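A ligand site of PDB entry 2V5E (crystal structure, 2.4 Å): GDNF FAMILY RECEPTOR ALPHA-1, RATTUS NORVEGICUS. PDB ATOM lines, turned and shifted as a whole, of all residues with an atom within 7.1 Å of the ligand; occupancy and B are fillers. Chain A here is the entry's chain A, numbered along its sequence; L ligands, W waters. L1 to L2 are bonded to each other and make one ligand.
O13 of LIG L1 is in salt-bridge range of NZ of Lys 45, at 2.7 Å. The side-chain amide nitrogen (NE2) of Gln 49 is in hydrogen-bond range of an oxygen (O13) of LG2 L2. O3 of LG2 L2 lies within salt-bridge range of NE of Arg 48 (2.7 Å). An oxygen (O8) of LIG L1 is in hydrogen-bond range of the side-chain amide nitrogen of Asn 104, 2.7 Å away. NZ of Lys 53 lies within salt-bridge range of O14 of LG2 L2, at 3.0 Å. The guanidinium group (NH1) of Arg 41 is in salt-bridge range of an oxygen (O11) of LIG L1 (3.0 Å). N of Ile 106 lies within hydrogen-bond range of O4 of LIG L1 (3.5 Å).
The guanidinium group (NH1) of Arg 48 lies within hydrogen-bond range of the backbone carbonyl oxygen (O) of Gly 145, at 2.9 Å. The side-chain amide oxygen of Asn 104 lies within hydrogen-bond range of the backbone NH of Ile 106. OD1 of Asn 104 lies within hydrogen-bond range of N of Cys 107 (2.9 Å).
Residues that only touch the ligand: Tyr 105. Hydrophobic or aromatic side chains that line the ligand: Tyr 105 and Ile 106.
Water W6 bridges O3 of LIG L1 (2.8 Å) and N of Tyr 105 (3.1 Å). Water W4 bridges an oxygen (O9) of LG2 L2 and the side-chain amino group of Lys 53. Water W3 lies within hydrogen-bond range of OD1 of Asn 104 (2.6 Å) and O9 of LIG L1 (3.1 Å). Water W5 lies within hydrogen-bond range of O of Arg 41 (2.7 Å), NH1 of Arg 48 (3.2 Å) and O12 of LIG L1 (3.4 Å).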
ATOM      1  N   ARG A  41       7.841  21.925  17.198  1.00  0.00           N
ATOM      2  CA  ARG A  41       8.629  23.013  16.611  1.00  0.00           C
ATOM      3  C   ARG A  41       8.769  24.204  17.568  1.00  0.00           C
ATOM      4  O   ARG A  41       9.867  24.720  17.781  1.00  0.00           O
ATOM      5  CB  ARG A  41       8.053  23.461  15.255  1.00  0.00           C
ATOM      6  CG  ARG A  41       8.743  24.705  14.663  1.00  0.00           C
ATOM      7  CD  ARG A  41       8.210  25.133  13.293  1.00  0.00           C
ATOM      8  NE  ARG A  41       7.057  26.027  13.379  1.00  0.00           N
ATOM      9  CZ  ARG A  41       7.019  27.126  14.126  1.00  0.00           C
ATOM     10  NH1 ARG A  41       8.049  27.457  14.877  1.00  0.00           N
ATOM     11  NH2 ARG A  41       5.931  27.875  14.143  1.00  0.00           N
ATOM     12  N   LYS A  42       7.657  24.660  18.130  1.00  0.00           N
ATOM     13  CA  LYS A  42       7.631  25.828  19.043  1.00  0.00           C
ATOM     14  C   LYS A  42       8.312  25.503  20.376  1.00  0.00           C
ATOM     15  O   LYS A  42       8.933  26.365  20.990  1.00  0.00           O
ATOM     16  CB  LYS A  42       6.202  26.279  19.331  1.00  0.00           C
ATOM     17  CG  LYS A  42       5.468  26.922  18.161  1.00  0.00           C
ATOM     18  CD  LYS A  42       4.161  27.583  18.652  1.00  0.00           C
ATOM     19  CE  LYS A  42       3.474  28.384  17.530  1.00  0.00           C
ATOM     20  NZ  LYS A  42       2.148  28.946  17.958  1.00  0.00           N
ATOM     21  N   HIS A  44      10.777  23.150  20.684  1.00  0.00           N
ATOM     22  CA  HIS A  44      12.183  23.155  20.253  1.00  0.00           C
ATOM     23  C   HIS A  44      12.776  24.564  20.179  1.00  0.00           C
ATOM     24  O   HIS A  44      13.835  24.828  20.768  1.00  0.00           O
ATOM     25  CB  HIS A  44      12.345  22.381  18.937  1.00  0.00           C
ATOM     26  CG  HIS A  44      12.460  20.896  19.117  1.00  0.00           C
ATOM     27  ND1 HIS A  44      12.694  20.033  18.060  1.00  0.00           N
ATOM     28  CD2 HIS A  44      12.412  20.122  20.236  1.00  0.00           C
ATOM     29  CE1 HIS A  44      12.780  18.790  18.525  1.00  0.00           C
ATOM     30  NE2 HIS A  44      12.611  18.817  19.829  1.00  0.00           N
ATOM     31  N   LYS A  45      12.062  25.465  19.519  1.00  0.00           N
ATOM     32  CA  LYS A  45      12.498  26.863  19.411  1.00  0.00           C
ATOM     33  C   LYS A  45      12.793  27.490  20.767  1.00  0.00           C
ATOM     34  O   LYS A  45      13.880  28.037  20.985  1.00  0.00           O
ATOM     35  CB  LYS A  45      11.444  27.689  18.665  1.00  0.00           C
ATOM     36  CG  LYS A  45      11.905  29.047  18.191  1.00  0.00           C
ATOM     37  CD  LYS A  45      10.779  29.729  17.443  1.00  0.00           C
ATOM     38  CE  LYS A  45      11.076  31.192  17.164  1.00  0.00           C
ATOM     39  NZ  LYS A  45      12.006  31.338  16.025  1.00  0.00           N
ATOM     40  N   ALA A  46      11.841  27.389  21.686  1.00  0.00           N
ATOM     41  CA  ALA A  46      11.981  27.985  23.000  1.00  0.00           C
ATOM     42  C   ALA A  46      13.121  27.339  23.795  1.00  0.00           C
ATOM     43  O   ALA A  46      13.819  28.019  24.557  1.00  0.00           O
ATOM     44  CB  ALA A  46      10.670  27.919  23.749  1.00  0.00           C
ATOM     45  N   LEU A  47      13.332  26.026  23.592  1.00  0.00           N
ATOM     46  CA  LEU A  47      14.470  25.332  24.221  1.00  0.00           C
ATOM     47  C   LEU A  47      15.819  25.884  23.756  1.00  0.00           C
ATOM     48  O   LEU A  47      16.696  26.127  24.583  1.00  0.00           O
ATOM     49  CB  LEU A  47      14.392  23.813  24.002  1.00  0.00           C
ATOM     50  CG  LEU A  47      13.425  23.047  24.931  1.00  0.00           C
ATOM     51  CD1 LEU A  47      13.101  21.688  24.338  1.00  0.00           C
ATOM     52  CD2 LEU A  47      14.002  22.885  26.317  1.00  0.00           C
ATOM     53  N   ARG A  48      15.958  26.067  22.447  1.00  0.00           N
ATOM     54  CA  ARG A  48      17.165  26.659  21.853  1.00  0.00           C
ATOM     55  C   ARG A  48      17.409  28.053  22.424  1.00  0.00           C
ATOM     56  O   ARG A  48      18.507  28.356  22.892  1.00  0.00           O
ATOM     57  CB  ARG A  48      17.070  26.716  20.322  1.00  0.00           C
ATOM     58  CG  ARG A  48      17.177  25.363  19.619  1.00  0.00           C
ATOM     59  CD  ARG A  48      17.418  25.497  18.102  1.00  0.00           C
ATOM     60  NE  ARG A  48      16.479  26.422  17.468  1.00  0.00           N
ATOM     61  CZ  ARG A  48      15.297  26.081  16.966  1.00  0.00           C
ATOM     62  NH1 ARG A  48      14.869  24.828  17.009  1.00  0.00           N
ATOM     63  NH2 ARG A  48      14.532  27.021  16.398  1.00  0.00           N
ATOM     64  N   GLN A  49      16.358  28.891  22.415  1.00  0.00           N
ATOM     65  CA  GLN A  49      16.452  30.231  23.008  1.00  0.00           C
ATOM     66  C   GLN A  49      16.823  30.200  24.482  1.00  0.00           C
ATOM     67  O   GLN A  49      17.624  31.030  24.915  1.00  0.00           O
ATOM     68  CB  GLN A  49      15.162  31.043  22.777  1.00  0.00           C
ATOM     69  CG  GLN A  49      14.768  31.151  21.282  1.00  0.00           C
ATOM     70  CD  GLN A  49      13.730  32.230  20.986  1.00  0.00           C
ATOM     71  OE1 GLN A  49      12.910  32.589  21.828  1.00  0.00           O
ATOM     72  NE2 GLN A  49      13.771  32.761  19.771  1.00  0.00           N
ATOM     73  N   ASP A  52      20.617  29.376  24.512  1.00  0.00           N
ATOM     74  CA  ASP A  52      21.374  30.433  23.835  1.00  0.00           C
ATOM     75  C   ASP A  52      21.323  31.754  24.598  1.00  0.00           C
ATOM     76  O   ASP A  52      22.288  32.502  24.591  1.00  0.00           O
ATOM     77  CB  ASP A  52      20.850  30.632  22.399  1.00  0.00           C
ATOM     78  CG  ASP A  52      21.775  31.494  21.537  1.00  0.00           C
ATOM     79  OD1 ASP A  52      23.016  31.266  21.520  1.00  0.00           O
ATOM     80  OD2 ASP A  52      21.235  32.391  20.854  1.00  0.00           O
ATOM     81  N   LYS A  53      20.211  32.022  25.280  1.00  0.00           N
ATOM     82  CA  LYS A  53      20.013  33.340  25.888  1.00  0.00           C
ATOM     83  C   LYS A  53      20.288  33.387  27.374  1.00  0.00           C
ATOM     84  O   LYS A  53      20.564  34.456  27.903  1.00  0.00           O
ATOM     85  CB  LYS A  53      18.635  33.906  25.553  1.00  0.00           C
ATOM     86  CG  LYS A  53      18.486  34.403  24.111  1.00  0.00           C
ATOM     87  CD  LYS A  53      19.738  35.207  23.681  1.00  0.00           C
ATOM     88  CE  LYS A  53      19.458  36.242  22.594  1.00  0.00           C
ATOM     89  NZ  LYS A  53      18.823  35.659  21.413  1.00  0.00           N
ATOM     90  N   THR A 103      20.631  18.472   7.091  1.00  0.00           N
ATOM     91  CA  THR A 103      19.961  19.394   6.150  1.00  0.00           C
ATOM     92  C   THR A 103      19.596  20.732   6.820  1.00  0.00           C
ATOM     93  O   THR A 103      19.112  21.655   6.169  1.00  0.00           O
ATOM     94  CB  THR A 103      18.661  18.796   5.553  1.00  0.00           C
ATOM     95  OG1 THR A 103      17.658  18.704   6.577  1.00  0.00           O
ATOM     96  CG2 THR A 103      18.915  17.389   4.930  1.00  0.00           C
ATOM     97  N   ASN A 104      19.835  20.828   8.126  1.00  0.00           N
ATOM     98  CA  ASN A 104      19.480  22.013   8.874  1.00  0.00           C
ATOM     99  C   ASN A 104      20.735  22.689   9.377  1.00  0.00           C
ATOM    100  O   ASN A 104      21.601  22.041   9.985  1.00  0.00           O
ATOM    101  CB  ASN A 104      18.558  21.670  10.054  1.00  0.00           C
ATOM    102  CG  ASN A 104      18.225  22.877  10.893  1.00  0.00           C
ATOM    103  OD1 ASN A 104      18.809  23.093  11.967  1.00  0.00           O
ATOM    104  ND2 ASN A 104      17.320  23.706  10.384  1.00  0.00           N
ATOM    105  N   TYR A 105      20.847  23.996   9.127  1.00  0.00           N
ATOM    106  CA  TYR A 105      22.087  24.701   9.443  1.00  0.00           C
ATOM    107  C   TYR A 105      22.453  24.561  10.928  1.00  0.00           C
ATOM    108  O   TYR A 105      23.588  24.225  11.256  1.00  0.00           O
ATOM    109  CB  TYR A 105      22.065  26.173   9.011  1.00  0.00           C
ATOM    110  CG  TYR A 105      23.100  26.977   9.752  1.00  0.00           C
ATOM    111  CD1 TYR A 105      24.471  26.807   9.488  1.00  0.00           C
ATOM    112  CD2 TYR A 105      22.729  27.896  10.739  1.00  0.00           C
ATOM    113  CE1 TYR A 105      25.435  27.512  10.183  1.00  0.00           C
ATOM    114  CE2 TYR A 105      23.693  28.602  11.444  1.00  0.00           C
ATOM    115  CZ  TYR A 105      25.046  28.410  11.160  1.00  0.00           C
ATOM    116  OH  TYR A 105      26.012  29.132  11.833  1.00  0.00           O
ATOM    117  N   ILE A 106      21.493  24.828  11.818  1.00  0.00           N
ATOM    118  CA  ILE A 106      21.787  24.800  13.253  1.00  0.00           C
ATOM    119  C   ILE A 106      22.126  23.366  13.712  1.00  0.00           C
ATOM    120  O   ILE A 106      23.120  23.147  14.418  1.00  0.00           O
ATOM    121  CB  ILE A 106      20.587  25.322  14.082  1.00  0.00           C
ATOM    122  CG1 ILE A 106      20.418  26.838  13.923  1.00  0.00           C
ATOM    123  CG2 ILE A 106      20.747  24.911  15.566  1.00  0.00           C
ATOM    124  CD1 ILE A 106      19.196  27.396  14.635  1.00  0.00           C
ATOM    125  N   CYS A 107      21.311  22.406  13.292  1.00  0.00           N
ATOM    126  CA  CYS A 107      21.564  21.020  13.677  1.00  0.00           C
ATOM    127  C   CYS A 107      22.923  20.532  13.174  1.00  0.00           C
ATOM    128  O   CYS A 107      23.734  20.031  13.962  1.00  0.00           O
ATOM    129  CB  CYS A 107      20.439  20.075  13.236  1.00  0.00           C
ATOM    130  SG  CYS A 107      20.445  18.542  14.209  1.00  0.00           S
ATOM    131  N   ARG A 110      25.710  22.285  15.315  1.00  0.00           N
ATOM    132  CA  ARG A 110      25.724  21.785  16.694  1.00  0.00           C
ATOM    133  C   ARG A 110      26.180  20.312  16.764  1.00  0.00           C
ATOM    134  O   ARG A 110      26.968  19.930  17.629  1.00  0.00           O
ATOM    135  CB  ARG A 110      24.339  21.946  17.341  1.00  0.00           C
ATOM    136  CG  ARG A 110      23.776  23.383  17.355  1.00  0.00           C
ATOM    137  CD  ARG A 110      24.452  24.278  18.345  1.00  0.00           C
ATOM    138  NE  ARG A 110      23.957  25.653  18.312  1.00  0.00           N
ATOM    139  CZ  ARG A 110      22.913  26.126  18.999  1.00  0.00           C
ATOM    140  NH1 ARG A 110      22.191  25.345  19.791  1.00  0.00           N
ATOM    141  NH2 ARG A 110      22.581  27.399  18.901  1.00  0.00           N
ATOM    142  N   GLY A 145      16.668  21.000  21.340  1.00  0.00           N
ATOM    143  CA  GLY A 145      15.860  21.801  20.449  1.00  0.00           C
ATOM    144  C   GLY A 145      16.168  21.569  18.968  1.00  0.00           C
ATOM    145  O   GLY A 145      15.623  22.265  18.114  1.00  0.00           O
ATOM    146  N   THR A 146      17.051  20.619  18.670  1.00  0.00           N
ATOM    147  CA  THR A 146      17.252  20.190  17.270  1.00  0.00           C
ATOM    148  C   THR A 146      16.595  18.825  17.131  1.00  0.00           C
ATOM    149  O   THR A 146      16.194  18.254  18.133  1.00  0.00           O
ATOM    150  CB  THR A 146      18.740  20.093  16.889  1.00  0.00           C
ATOM    151  OG1 THR A 146      19.326  18.963  17.541  1.00  0.00           O
ATOM    152  CG2 THR A 146      19.498  21.361  17.291  1.00  0.00           C
HETATM  153  C1  LIG L   1      15.215  31.444  12.615  1.00  0.00           C
HETATM  154  O1  LIG L   1      16.237  30.649  12.021  1.00  0.00           O
HETATM  155  C2  LIG L   1      16.335  29.322  12.637  1.00  0.00           C
HETATM  156  C3  LIG L   1      17.498  28.608  11.998  1.00  0.00           C
HETATM  157  O2  LIG L   1      17.330  28.493  10.589  1.00  0.00           O
HETATM  158  S1  LIG L   1      18.462  28.119   9.758  1.00  0.00           S
HETATM  159  O3  LIG L   1      17.978  27.919   8.339  1.00  0.00           O
HETATM  160  O4  LIG L   1      19.058  26.815  10.289  1.00  0.00           O
HETATM  161  O5  LIG L   1      19.543  29.212   9.816  1.00  0.00           O
HETATM  162  C4  LIG L   1      15.026  28.530  12.475  1.00  0.00           C
HETATM  163  O6  LIG L   1      15.072  27.319  13.255  1.00  0.00           O
HETATM  164  S2  LIG L   1      15.059  26.011  12.637  1.00  0.00           S
HETATM  165  O7  LIG L   1      13.908  25.880  11.651  1.00  0.00           O
HETATM  166  O8  LIG L   1      16.355  25.785  11.897  1.00  0.00           O
HETATM  167  O9  LIG L   1      14.946  24.970  13.737  1.00  0.00           O
HETATM  168  C5  LIG L   1      13.856  29.353  13.011  1.00  0.00           C
HETATM  169  O10 LIG L   1      12.631  28.606  12.771  1.00  0.00           O
HETATM  170  S3  LIG L   1      11.584  28.403  13.803  1.00  0.00           S
HETATM  171  O11 LIG L   1      10.531  27.503  13.202  1.00  0.00           O
HETATM  172  O12 LIG L   1      12.177  27.775  15.070  1.00  0.00           O
HETATM  173  O13 LIG L   1      10.942  29.737  14.195  1.00  0.00           O
HETATM  174  C6  LIG L   1      13.845  30.763  12.384  1.00  0.00           C
HETATM  175  O14 LIG L   1      12.820  31.590  12.985  1.00  0.00           O
HETATM  176  S4  LIG L   1      12.016  32.542  12.179  1.00  0.00           S
HETATM  177  O15 LIG L   1      11.294  31.762  11.082  1.00  0.00           O
HETATM  178  O16 LIG L   1      11.011  33.251  13.077  1.00  0.00           O
HETATM  179  O17 LIG L   1      12.932  33.570  11.551  1.00  0.00           O
HETATM  180  C1  LG2 L   2      15.290  34.028  14.437  1.00  0.00           C
HETATM  181  C2  LG2 L   2      16.187  32.758  14.518  1.00  0.00           C
HETATM  182  C3  LG2 L   2      16.630  32.537  15.979  1.00  0.00           C
HETATM  183  C4  LG2 L   2      17.994  33.212  16.058  1.00  0.00           C
HETATM  184  C5  LG2 L   2      18.564  32.992  14.672  1.00  0.00           C
HETATM  185  C6  LG2 L   2      19.442  31.720  14.741  1.00  0.00           C
HETATM  186  O1  LG2 L   2      14.029  33.858  15.142  1.00  0.00           O
HETATM  187  O2  LG2 L   2      12.838  35.939  14.592  1.00  0.00           O
HETATM  188  O3  LG2 L   2      16.603  29.149  17.673  1.00  0.00           O
HETATM  189  O4  LG2 L   2      20.074  34.978  17.333  1.00  0.00           O
HETATM  190  O5  LG2 L   2      22.353  31.319  14.044  1.00  0.00           O
HETATM  191  O6  LG2 L   2      15.501  31.576  14.043  1.00  0.00           O
HETATM  192  O7  LG2 L   2      12.048  34.477  16.430  1.00  0.00           O
HETATM  193  O8  LG2 L   2      14.788  29.800  16.105  1.00  0.00           O
HETATM  194  O9  LG2 L   2      18.350  36.758  17.188  1.00  0.00           O
HETATM  195  O10 LG2 L   2      21.498  31.389  11.671  1.00  0.00           O
HETATM  196  O11 LG2 L   2      16.792  31.126  16.267  1.00  0.00           O
HETATM  197  O12 LG2 L   2      14.166  35.779  16.687  1.00  0.00           O
HETATM  198  O13 LG2 L   2      15.175  31.178  18.106  1.00  0.00           O
HETATM  199  O14 LG2 L   2      18.050  34.807  18.691  1.00  0.00           O
HETATM  200  O15 LG2 L   2      21.367  33.379  13.132  1.00  0.00           O
HETATM  201  O16 LG2 L   2      17.888  34.611  16.272  1.00  0.00           O
HETATM  202  O17 LG2 L   2      17.405  32.898  13.752  1.00  0.00           O
HETATM  203  O18 LG2 L   2      19.996  31.412  13.474  1.00  0.00           O
HETATM  204  S1  LG2 L   2      13.290  35.007  15.716  1.00  0.00           S
HETATM  205  S2  LG2 L   2      15.851  30.324  17.040  1.00  0.00           S
HETATM  206  S3  LG2 L   2      18.589  35.266  17.350  1.00  0.00           S
HETATM  207  S4  LG2 L   2      21.293  31.861  13.096  1.00  0.00           S
HETATM  208  O   HOH W   1      20.906  29.285   7.485  1.00  0.00           O
HETATM  209  O   HOH W   2      16.345  37.718  15.760  1.00  0.00           O
HETATM  210  O   HOH W   3      17.405  23.179  14.207  1.00  0.00           O
HETATM  211  O   HOH W   4      18.422  38.070  19.711  1.00  0.00           O
HETATM  212  O   HOH W   5      11.881  24.501  15.998  1.00  0.00           O
HETATM  213  O   HOH W   6      18.728  25.415   7.346  1.00  0.00           O
HETATM  214  O   HOH W   7      15.115  36.899  13.517  1.00  0.00           O
